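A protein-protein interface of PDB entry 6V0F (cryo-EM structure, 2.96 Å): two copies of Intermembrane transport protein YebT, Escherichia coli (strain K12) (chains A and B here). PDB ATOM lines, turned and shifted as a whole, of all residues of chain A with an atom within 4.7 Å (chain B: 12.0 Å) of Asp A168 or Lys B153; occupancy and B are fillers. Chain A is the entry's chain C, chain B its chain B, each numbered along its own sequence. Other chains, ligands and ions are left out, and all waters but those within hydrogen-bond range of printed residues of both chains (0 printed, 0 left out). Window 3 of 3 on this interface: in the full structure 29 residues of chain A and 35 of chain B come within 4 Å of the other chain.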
ATOM      1  N   PHE A 136     -33.871 -26.674   7.933  1.00  0.00           N
ATOM      2  CA  PHE A 136     -33.417 -28.017   8.255  1.00  0.00           C
ATOM      3  C   PHE A 136     -33.864 -28.283   9.673  1.00  0.00           C
ATOM      4  O   PHE A 136     -33.470 -27.548  10.581  1.00  0.00           O
ATOM      5  CB  PHE A 136     -31.901 -28.159   8.162  1.00  0.00           C
ATOM      6  CG  PHE A 136     -31.405 -29.533   8.506  1.00  0.00           C
ATOM      7  CD1 PHE A 136     -31.475 -30.546   7.582  1.00  0.00           C
ATOM      8  CD2 PHE A 136     -30.877 -29.812   9.755  1.00  0.00           C
ATOM      9  CE1 PHE A 136     -31.028 -31.804   7.886  1.00  0.00           C
ATOM     10  CE2 PHE A 136     -30.421 -31.072  10.060  1.00  0.00           C
ATOM     11  CZ  PHE A 136     -30.499 -32.069   9.125  1.00  0.00           C
ATOM     12  N   ARG A 137     -34.682 -29.328   9.848  1.00  0.00           N
ATOM     13  CA  ARG A 137     -35.335 -29.665  11.115  1.00  0.00           C
ATOM     14  C   ARG A 137     -36.138 -28.482  11.650  1.00  0.00           C
ATOM     15  O   ARG A 137     -36.177 -28.235  12.855  1.00  0.00           O
ATOM     16  CB  ARG A 137     -34.332 -30.148  12.155  1.00  0.00           C
ATOM     17  CG  ARG A 137     -33.554 -31.389  11.808  1.00  0.00           C
ATOM     18  CD  ARG A 137     -34.373 -32.638  11.942  1.00  0.00           C
ATOM     19  NE  ARG A 137     -33.561 -33.826  11.714  1.00  0.00           N
ATOM     20  CZ  ARG A 137     -34.034 -35.065  11.719  1.00  0.00           C
ATOM     21  NH1 ARG A 137     -35.317 -35.284  11.944  1.00  0.00           N
ATOM     22  NH2 ARG A 137     -33.221 -36.087  11.499  1.00  0.00           N
ATOM     23  N   ARG A 165     -21.978 -21.673   8.049  1.00  0.00           N
ATOM     24  CA  ARG A 165     -21.943 -22.660   9.127  1.00  0.00           C
ATOM     25  C   ARG A 165     -22.500 -24.004   8.682  1.00  0.00           C
ATOM     26  O   ARG A 165     -21.992 -25.058   9.079  1.00  0.00           O
ATOM     27  CB  ARG A 165     -22.739 -22.182  10.336  1.00  0.00           C
ATOM     28  CG  ARG A 165     -22.186 -21.000  11.060  1.00  0.00           C
ATOM     29  CD  ARG A 165     -23.096 -20.670  12.221  1.00  0.00           C
ATOM     30  NE  ARG A 165     -24.395 -20.167  11.797  1.00  0.00           N
ATOM     31  CZ  ARG A 165     -25.399 -19.934  12.632  1.00  0.00           C
ATOM     32  NH1 ARG A 165     -25.244 -20.165  13.927  1.00  0.00           N
ATOM     33  NH2 ARG A 165     -26.555 -19.473  12.180  1.00  0.00           N
ATOM     34  N   PHE A 166     -23.547 -23.984   7.863  1.00  0.00           N
ATOM     35  CA  PHE A 166     -24.335 -25.168   7.568  1.00  0.00           C
ATOM     36  C   PHE A 166     -23.982 -25.800   6.230  1.00  0.00           C
ATOM     37  O   PHE A 166     -24.807 -26.518   5.663  1.00  0.00           O
ATOM     38  CB  PHE A 166     -25.815 -24.805   7.592  1.00  0.00           C
ATOM     39  CG  PHE A 166     -26.259 -24.190   8.879  1.00  0.00           C
ATOM     40  CD1 PHE A 166     -26.502 -24.967   9.991  1.00  0.00           C
ATOM     41  CD2 PHE A 166     -26.442 -22.824   8.971  1.00  0.00           C
ATOM     42  CE1 PHE A 166     -26.913 -24.392  11.175  1.00  0.00           C
ATOM     43  CE2 PHE A 166     -26.852 -22.245  10.148  1.00  0.00           C
ATOM     44  CZ  PHE A 166     -27.089 -23.030  11.250  1.00  0.00           C
ATOM     45  N   THR A 167     -22.783 -25.537   5.705  1.00  0.00           N
ATOM     46  CA  THR A 167     -22.371 -26.139   4.439  1.00  0.00           C
ATOM     47  C   THR A 167     -22.205 -27.648   4.544  1.00  0.00           C
ATOM     48  O   THR A 167     -22.368 -28.359   3.548  1.00  0.00           O
ATOM     49  CB  THR A 167     -21.066 -25.518   3.957  1.00  0.00           C
ATOM     50  OG1 THR A 167     -20.050 -25.719   4.947  1.00  0.00           O
ATOM     51  CG2 THR A 167     -21.239 -24.041   3.714  1.00  0.00           C
ATOM     52  N   ASP A 168     -21.873 -28.153   5.726  1.00  0.00           N
ATOM     53  CA  ASP A 168     -21.734 -29.586   5.926  1.00  0.00           C
ATOM     54  C   ASP A 168     -23.064 -30.316   6.055  1.00  0.00           C
ATOM     55  O   ASP A 168     -23.072 -31.549   6.060  1.00  0.00           O
ATOM     56  CB  ASP A 168     -20.869 -29.841   7.163  1.00  0.00           C
ATOM     57  CG  ASP A 168     -21.373 -29.107   8.395  1.00  0.00           C
ATOM     58  OD1 ASP A 168     -22.313 -28.296   8.269  1.00  0.00           O
ATOM     59  OD2 ASP A 168     -20.821 -29.330   9.492  1.00  0.00           O
ATOM     60  N   LEU A 169     -24.175 -29.593   6.177  1.00  0.00           N
ATOM     61  CA  LEU A 169     -25.482 -30.236   6.252  1.00  0.00           C
ATOM     62  C   LEU A 169     -25.906 -30.796   4.902  1.00  0.00           C
ATOM     63  O   LEU A 169     -26.387 -31.930   4.813  1.00  0.00           O
ATOM     64  CB  LEU A 169     -26.526 -29.248   6.763  1.00  0.00           C
ATOM     65  CG  LEU A 169     -26.769 -29.106   8.261  1.00  0.00           C
ATOM     66  CD1 LEU A 169     -25.597 -28.497   8.981  1.00  0.00           C
ATOM     67  CD2 LEU A 169     -27.974 -28.238   8.450  1.00  0.00           C
ATOM     68  N   VAL A 170     -25.749 -30.007   3.842  1.00  0.00           N
ATOM     69  CA  VAL A 170     -26.197 -30.394   2.511  1.00  0.00           C
ATOM     70  C   VAL A 170     -25.301 -31.492   1.956  1.00  0.00           C
ATOM     71  O   VAL A 170     -24.105 -31.281   1.725  1.00  0.00           O
ATOM     72  CB  VAL A 170     -26.216 -29.182   1.577  1.00  0.00           C
ATOM     73  CG1 VAL A 170     -26.572 -29.614   0.183  1.00  0.00           C
ATOM     74  CG2 VAL A 170     -27.196 -28.164   2.079  1.00  0.00           C
ATOM     75  N   LYS A 171     -25.878 -32.663   1.723  1.00  0.00           N
ATOM     76  CA  LYS A 171     -25.162 -33.809   1.187  1.00  0.00           C
ATOM     77  C   LYS A 171     -25.525 -34.003  -0.281  1.00  0.00           C
ATOM     78  O   LYS A 171     -26.424 -33.352  -0.810  1.00  0.00           O
ATOM     79  CB  LYS A 171     -25.496 -35.066   1.988  1.00  0.00           C
ATOM     80  CG  LYS A 171     -25.154 -34.960   3.456  1.00  0.00           C
ATOM     81  CD  LYS A 171     -23.667 -34.935   3.690  1.00  0.00           C
ATOM     82  CE  LYS A 171     -23.379 -34.832   5.169  1.00  0.00           C
ATOM     83  NZ  LYS A 171     -23.771 -36.071   5.887  1.00  0.00           N
ATOM     84  N   GLN B 121     -34.203 -31.887  24.184  1.00  0.00           N
ATOM     85  CA  GLN B 121     -33.835 -32.574  22.955  1.00  0.00           C
ATOM     86  C   GLN B 121     -35.107 -32.901  22.197  1.00  0.00           C
ATOM     87  O   GLN B 121     -35.928 -33.697  22.658  1.00  0.00           O
ATOM     88  CB  GLN B 121     -33.023 -33.827  23.238  1.00  0.00           C
ATOM     89  CG  GLN B 121     -31.652 -33.531  23.775  1.00  0.00           C
ATOM     90  CD  GLN B 121     -30.850 -34.783  24.003  1.00  0.00           C
ATOM     91  OE1 GLN B 121     -31.353 -35.893  23.830  1.00  0.00           O
ATOM     92  NE2 GLN B 121     -29.592 -34.619  24.396  1.00  0.00           N
ATOM     93  N   ALA B 122     -35.268 -32.279  21.045  1.00  0.00           N
ATOM     94  CA  ALA B 122     -36.423 -32.479  20.207  1.00  0.00           C
ATOM     95  C   ALA B 122     -35.984 -33.023  18.856  1.00  0.00           C
ATOM     96  O   ALA B 122     -34.866 -32.743  18.413  1.00  0.00           O
ATOM     97  CB  ALA B 122     -37.179 -31.159  20.024  1.00  0.00           C
ATOM     98  N   PRO B 123     -36.821 -33.816  18.182  1.00  0.00           N
ATOM     99  CA  PRO B 123     -36.434 -34.303  16.854  1.00  0.00           C
ATOM    100  C   PRO B 123     -36.454 -33.222  15.800  1.00  0.00           C
ATOM    101  O   PRO B 123     -35.807 -33.387  14.763  1.00  0.00           O
ATOM    102  CB  PRO B 123     -37.472 -35.387  16.559  1.00  0.00           C
ATOM    103  CG  PRO B 123     -38.646 -34.999  17.365  1.00  0.00           C
ATOM    104  CD  PRO B 123     -38.109 -34.386  18.614  1.00  0.00           C
ATOM    105  N   ASP B 124     -37.184 -32.135  16.023  1.00  0.00           N
ATOM    106  CA  ASP B 124     -37.141 -30.962  15.167  1.00  0.00           C
ATOM    107  C   ASP B 124     -37.532 -29.753  16.002  1.00  0.00           C
ATOM    108  O   ASP B 124     -38.050 -29.887  17.109  1.00  0.00           O
ATOM    109  CB  ASP B 124     -38.044 -31.108  13.941  1.00  0.00           C
ATOM    110  CG  ASP B 124     -39.475 -31.474  14.296  1.00  0.00           C
ATOM    111  OD1 ASP B 124     -39.769 -31.751  15.477  1.00  0.00           O
ATOM    112  OD2 ASP B 124     -40.325 -31.463  13.380  1.00  0.00           O
ATOM    113  N   LEU B 125     -37.277 -28.567  15.456  1.00  0.00           N
ATOM    114  CA  LEU B 125     -37.509 -27.340  16.208  1.00  0.00           C
ATOM    115  C   LEU B 125     -38.997 -27.085  16.402  1.00  0.00           C
ATOM    116  O   LEU B 125     -39.417 -26.610  17.461  1.00  0.00           O
ATOM    117  CB  LEU B 125     -36.835 -26.161  15.508  1.00  0.00           C
ATOM    118  CG  LEU B 125     -36.892 -24.820  16.230  1.00  0.00           C
ATOM    119  CD1 LEU B 125     -36.118 -24.919  17.500  1.00  0.00           C
ATOM    120  CD2 LEU B 125     -36.316 -23.715  15.384  1.00  0.00           C
ATOM    121  N   TYR B 147     -31.311 -22.286  20.246  1.00  0.00           N
ATOM    122  CA  TYR B 147     -31.516 -23.577  19.621  1.00  0.00           C
ATOM    123  C   TYR B 147     -30.317 -23.861  18.741  1.00  0.00           C
ATOM    124  O   TYR B 147     -29.770 -22.954  18.115  1.00  0.00           O
ATOM    125  CB  TYR B 147     -32.814 -23.614  18.810  1.00  0.00           C
ATOM    126  CG  TYR B 147     -32.960 -22.509  17.795  1.00  0.00           C
ATOM    127  CD1 TYR B 147     -33.578 -21.317  18.134  1.00  0.00           C
ATOM    128  CD2 TYR B 147     -32.490 -22.656  16.501  1.00  0.00           C
ATOM    129  CE1 TYR B 147     -33.721 -20.298  17.215  1.00  0.00           C
ATOM    130  CE2 TYR B 147     -32.618 -21.641  15.578  1.00  0.00           C
ATOM    131  CZ  TYR B 147     -33.237 -20.465  15.940  1.00  0.00           C
ATOM    132  OH  TYR B 147     -33.373 -19.454  15.017  1.00  0.00           O
ATOM    133  N   ALA B 148     -29.921 -25.123  18.694  1.00  0.00           N
ATOM    134  CA  ALA B 148     -28.725 -25.504  17.972  1.00  0.00           C
ATOM    135  C   ALA B 148     -28.820 -26.975  17.628  1.00  0.00           C
ATOM    136  O   ALA B 148     -29.368 -27.760  18.402  1.00  0.00           O
ATOM    137  CB  ALA B 148     -27.462 -25.238  18.795  1.00  0.00           C
ATOM    138  N   ILE B 149     -28.303 -27.336  16.475  1.00  0.00           N
ATOM    139  CA  ILE B 149     -28.238 -28.743  16.122  1.00  0.00           C
ATOM    140  C   ILE B 149     -27.100 -29.350  16.925  1.00  0.00           C
ATOM    141  O   ILE B 149     -26.018 -28.764  17.028  1.00  0.00           O
ATOM    142  CB  ILE B 149     -28.010 -28.901  14.611  1.00  0.00           C
ATOM    143  CG1 ILE B 149     -29.132 -28.225  13.841  1.00  0.00           C
ATOM    144  CG2 ILE B 149     -27.966 -30.354  14.224  1.00  0.00           C
ATOM    145  CD1 ILE B 149     -28.856 -28.108  12.376  1.00  0.00           C
ATOM    146  N   ASN B 150     -27.332 -30.528  17.498  1.00  0.00           N
ATOM    147  CA  ASN B 150     -26.306 -31.218  18.265  1.00  0.00           C
ATOM    148  C   ASN B 150     -25.288 -31.820  17.271  1.00  0.00           C
ATOM    149  O   ASN B 150     -25.500 -31.709  16.061  1.00  0.00           O
ATOM    150  CB  ASN B 150     -27.020 -32.137  19.284  1.00  0.00           C
ATOM    151  CG  ASN B 150     -27.762 -33.312  18.682  1.00  0.00           C
ATOM    152  OD1 ASN B 150     -27.259 -34.036  17.850  1.00  0.00           O
ATOM    153  ND2 ASN B 150     -29.002 -33.489  19.116  1.00  0.00           N
ATOM    154  N   PRO B 151     -24.128 -32.367  17.732  1.00  0.00           N
ATOM    155  CA  PRO B 151     -23.116 -32.861  16.759  1.00  0.00           C
ATOM    156  C   PRO B 151     -23.597 -33.868  15.729  1.00  0.00           C
ATOM    157  O   PRO B 151     -23.265 -33.721  14.547  1.00  0.00           O
ATOM    158  CB  PRO B 151     -22.015 -33.439  17.658  1.00  0.00           C
ATOM    159  CG  PRO B 151     -22.138 -32.712  18.905  1.00  0.00           C
ATOM    160  CD  PRO B 151     -23.576 -32.436  19.104  1.00  0.00           C
ATOM    161  N   ASN B 152     -24.337 -34.891  16.128  1.00  0.00           N
ATOM    162  CA  ASN B 152     -24.947 -35.729  15.113  1.00  0.00           C
ATOM    163  C   ASN B 152     -26.102 -34.928  14.506  1.00  0.00           C
ATOM    164  O   ASN B 152     -26.735 -34.112  15.167  1.00  0.00           O
ATOM    165  CB  ASN B 152     -25.414 -37.048  15.731  1.00  0.00           C
ATOM    166  CG  ASN B 152     -25.885 -38.071  14.699  1.00  0.00           C
ATOM    167  OD1 ASN B 152     -26.180 -37.756  13.547  1.00  0.00           O
ATOM    168  ND2 ASN B 152     -25.938 -39.327  15.126  1.00  0.00           N
ATOM    169  N   LYS B 153     -26.340 -35.122  13.216  1.00  0.00           N
ATOM    170  CA  LYS B 153     -27.404 -34.386  12.539  1.00  0.00           C
ATOM    171  C   LYS B 153     -28.817 -34.804  12.951  1.00  0.00           C
ATOM    172  O   LYS B 153     -29.769 -34.094  12.612  1.00  0.00           O
ATOM    173  CB  LYS B 153     -27.212 -34.520  11.035  1.00  0.00           C
ATOM    174  CG  LYS B 153     -25.812 -34.098  10.639  1.00  0.00           C
ATOM    175  CD  LYS B 153     -25.568 -32.636  10.958  1.00  0.00           C
ATOM    176  CE  LYS B 153     -24.189 -32.194  10.512  1.00  0.00           C
ATOM    177  NZ  LYS B 153     -23.938 -30.771  10.862  1.00  0.00           N
ATOM    178  N   GLN B 154     -28.958 -35.960  13.611  1.00  0.00           N
ATOM    179  CA  GLN B 154     -30.240 -36.540  14.030  1.00  0.00           C
ATOM    180  C   GLN B 154     -31.225 -35.596  14.730  1.00  0.00           C
ATOM    181  O   GLN B 154     -32.385 -35.500  14.318  1.00  0.00           O
ATOM    182  CB  GLN B 154     -29.969 -37.743  14.929  1.00  0.00           C
ATOM    183  CG  GLN B 154     -29.270 -38.871  14.215  1.00  0.00           C
ATOM    184  CD  GLN B 154     -30.117 -39.460  13.110  1.00  0.00           C
ATOM    185  OE1 GLN B 154     -29.916 -39.160  11.933  1.00  0.00           O
ATOM    186  NE2 GLN B 154     -31.076 -40.300  13.481  1.00  0.00           N
ATOM    187  N   GLY B 155     -30.809 -34.887  15.777  1.00  0.00           N
ATOM    188  CA  GLY B 155     -31.764 -34.111  16.545  1.00  0.00           C
ATOM    189  C   GLY B 155     -31.317 -32.713  16.919  1.00  0.00           C
ATOM    190  O   GLY B 155     -30.133 -32.382  16.926  1.00  0.00           O
ATOM    191  N   VAL B 156     -32.322 -31.890  17.208  1.00  0.00           N
ATOM    192  CA  VAL B 156     -32.165 -30.488  17.577  1.00  0.00           C
ATOM    193  C   VAL B 156     -32.220 -30.306  19.082  1.00  0.00           C
ATOM    194  O   VAL B 156     -33.173 -30.751  19.732  1.00  0.00           O
ATOM    195  CB  VAL B 156     -33.249 -29.643  16.906  1.00  0.00           C
ATOM    196  CG1 VAL B 156     -33.182 -28.216  17.372  1.00  0.00           C
ATOM    197  CG2 VAL B 156     -33.046 -29.721  15.466  1.00  0.00           C
ATOM    198  N   VAL B 157     -31.208 -29.651  19.642  1.00  0.00           N
ATOM    199  CA  VAL B 157     -31.179 -29.311  21.059  1.00  0.00           C
ATOM    200  C   VAL B 157     -31.630 -27.868  21.212  1.00  0.00           C
ATOM    201  O   VAL B 157     -31.024 -26.956  20.644  1.00  0.00           O
ATOM    202  CB  VAL B 157     -29.789 -29.525  21.668  1.00  0.00           C
ATOM    203  CG1 VAL B 157     -29.770 -29.035  23.084  1.00  0.00           C
ATOM    204  CG2 VAL B 157     -29.485 -30.987  21.682  1.00  0.00           C
ATOM    205  N   ILE B 158     -32.676 -27.661  22.001  1.00  0.00           N
ATOM    206  CA  ILE B 158     -33.244 -26.350  22.271  1.00  0.00           C
ATOM    207  C   ILE B 158     -32.959 -26.078  23.730  1.00  0.00           C
ATOM    208  O   ILE B 158     -33.505 -26.767  24.594  1.00  0.00           O
ATOM    209  CB  ILE B 158     -34.757 -26.347  22.047  1.00  0.00           C
ATOM    210  CG1 ILE B 158     -35.105 -26.720  20.622  1.00  0.00           C
ATOM    211  CG2 ILE B 158     -35.331 -25.018  22.402  1.00  0.00           C
ATOM    212  CD1 ILE B 158     -36.549 -27.075  20.481  1.00  0.00           C
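The side-chain amino group (NZ) of Lys B153 is in salt-bridge range of the side-chain carboxylate (OD2) of Asp A168. The backbone NH (N) of Leu B125 lies within hydrogen-bond range of the backbone carbonyl oxygen (O) of Arg A137. The guanidinium group (NH2) of Arg A137 lies within hydrogen-bond range of the backbone carbonyl oxygen (O) of Gln B154 (3.0 Å). The backbone carbonyl oxygen (O) of Pro B123 sits close to the guanidinium group (NH1) of Arg A137.
The backbone carbonyl oxygen (O) of Val B156 lies within hydrogen-bond range of the backbone NH (N) of Ala B122. The side-chain amide oxygen (OD1) of Asn B152 lies close to the backbone NH (N) of Gln B154, at 3.3 Å.
Phe A136 touches Ile B149 (CD2 to CD1, 3.7 Å). CB of Asp B124 touches O of Arg A137, 3.6 Å away. Arg A137 touches Lys B153 (NE to O, 3.9 Å). Val B156 touches Arg A137. CD1 of Leu A169 touches NZ of Lys B153, at 3.4 Å.
Asp A168 touches just one residue of chain B: Lys B153 (3.7 Å). Printed residues of chain A within 4 Å of Lys B153: Arg A137, Asp A168 and Leu A169. No residue of chain B comes within 4 Å of Phe A166. Of chain B, only Lys B153 comes within 4 Å of Leu A169. No residue of chain B comes within 4 Å of Val A170. Printed residues of chain A within 4 Å of Asp B124: Arg A137. Of the printed residues of chain B, Arg A137 touches Pro B123 (3.3 Å), Asp B124 (3.6 Å), Leu B125 (2.8 Å), Lys B153 (3.9 Å), Gln B154 (3.0 Å) and Val B156 (3.6 Å). Printed residues of chain A within 4 Å of Pro B123: Arg A137. Of the printed residues of chain A, Leu B125 touches Arg A137 (2.8 Å). Gly B155 touches none of the printed residues of chain A. The nearest residue of chain B that does not touch Asp A168 is Pro B151 (7.1 Å). The nearest printed residue of chain A that does not touch Val B156 is Phe A136 (5.4 Å).
Of the 9 printed residues of chain A, 4 touch a printed residue of chain B. Hydrophobic or aromatic side chains of chain A within 4 Å of the printed part of chain B: Phe A136 and Leu A169. Of the 17 printed residues of chain B, 7 touch a printed residue of chain A. Among the printed residues, Asp or Glu carboxylates within 4 Å of a Lys or Arg side-chain nitrogen of the other chain: Asp A168 with Lys B153.
No position is printed for both chains. Of the 9 pairs that touch across the chains among the printed residues, none has its exchanged pair printed and touching as well.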
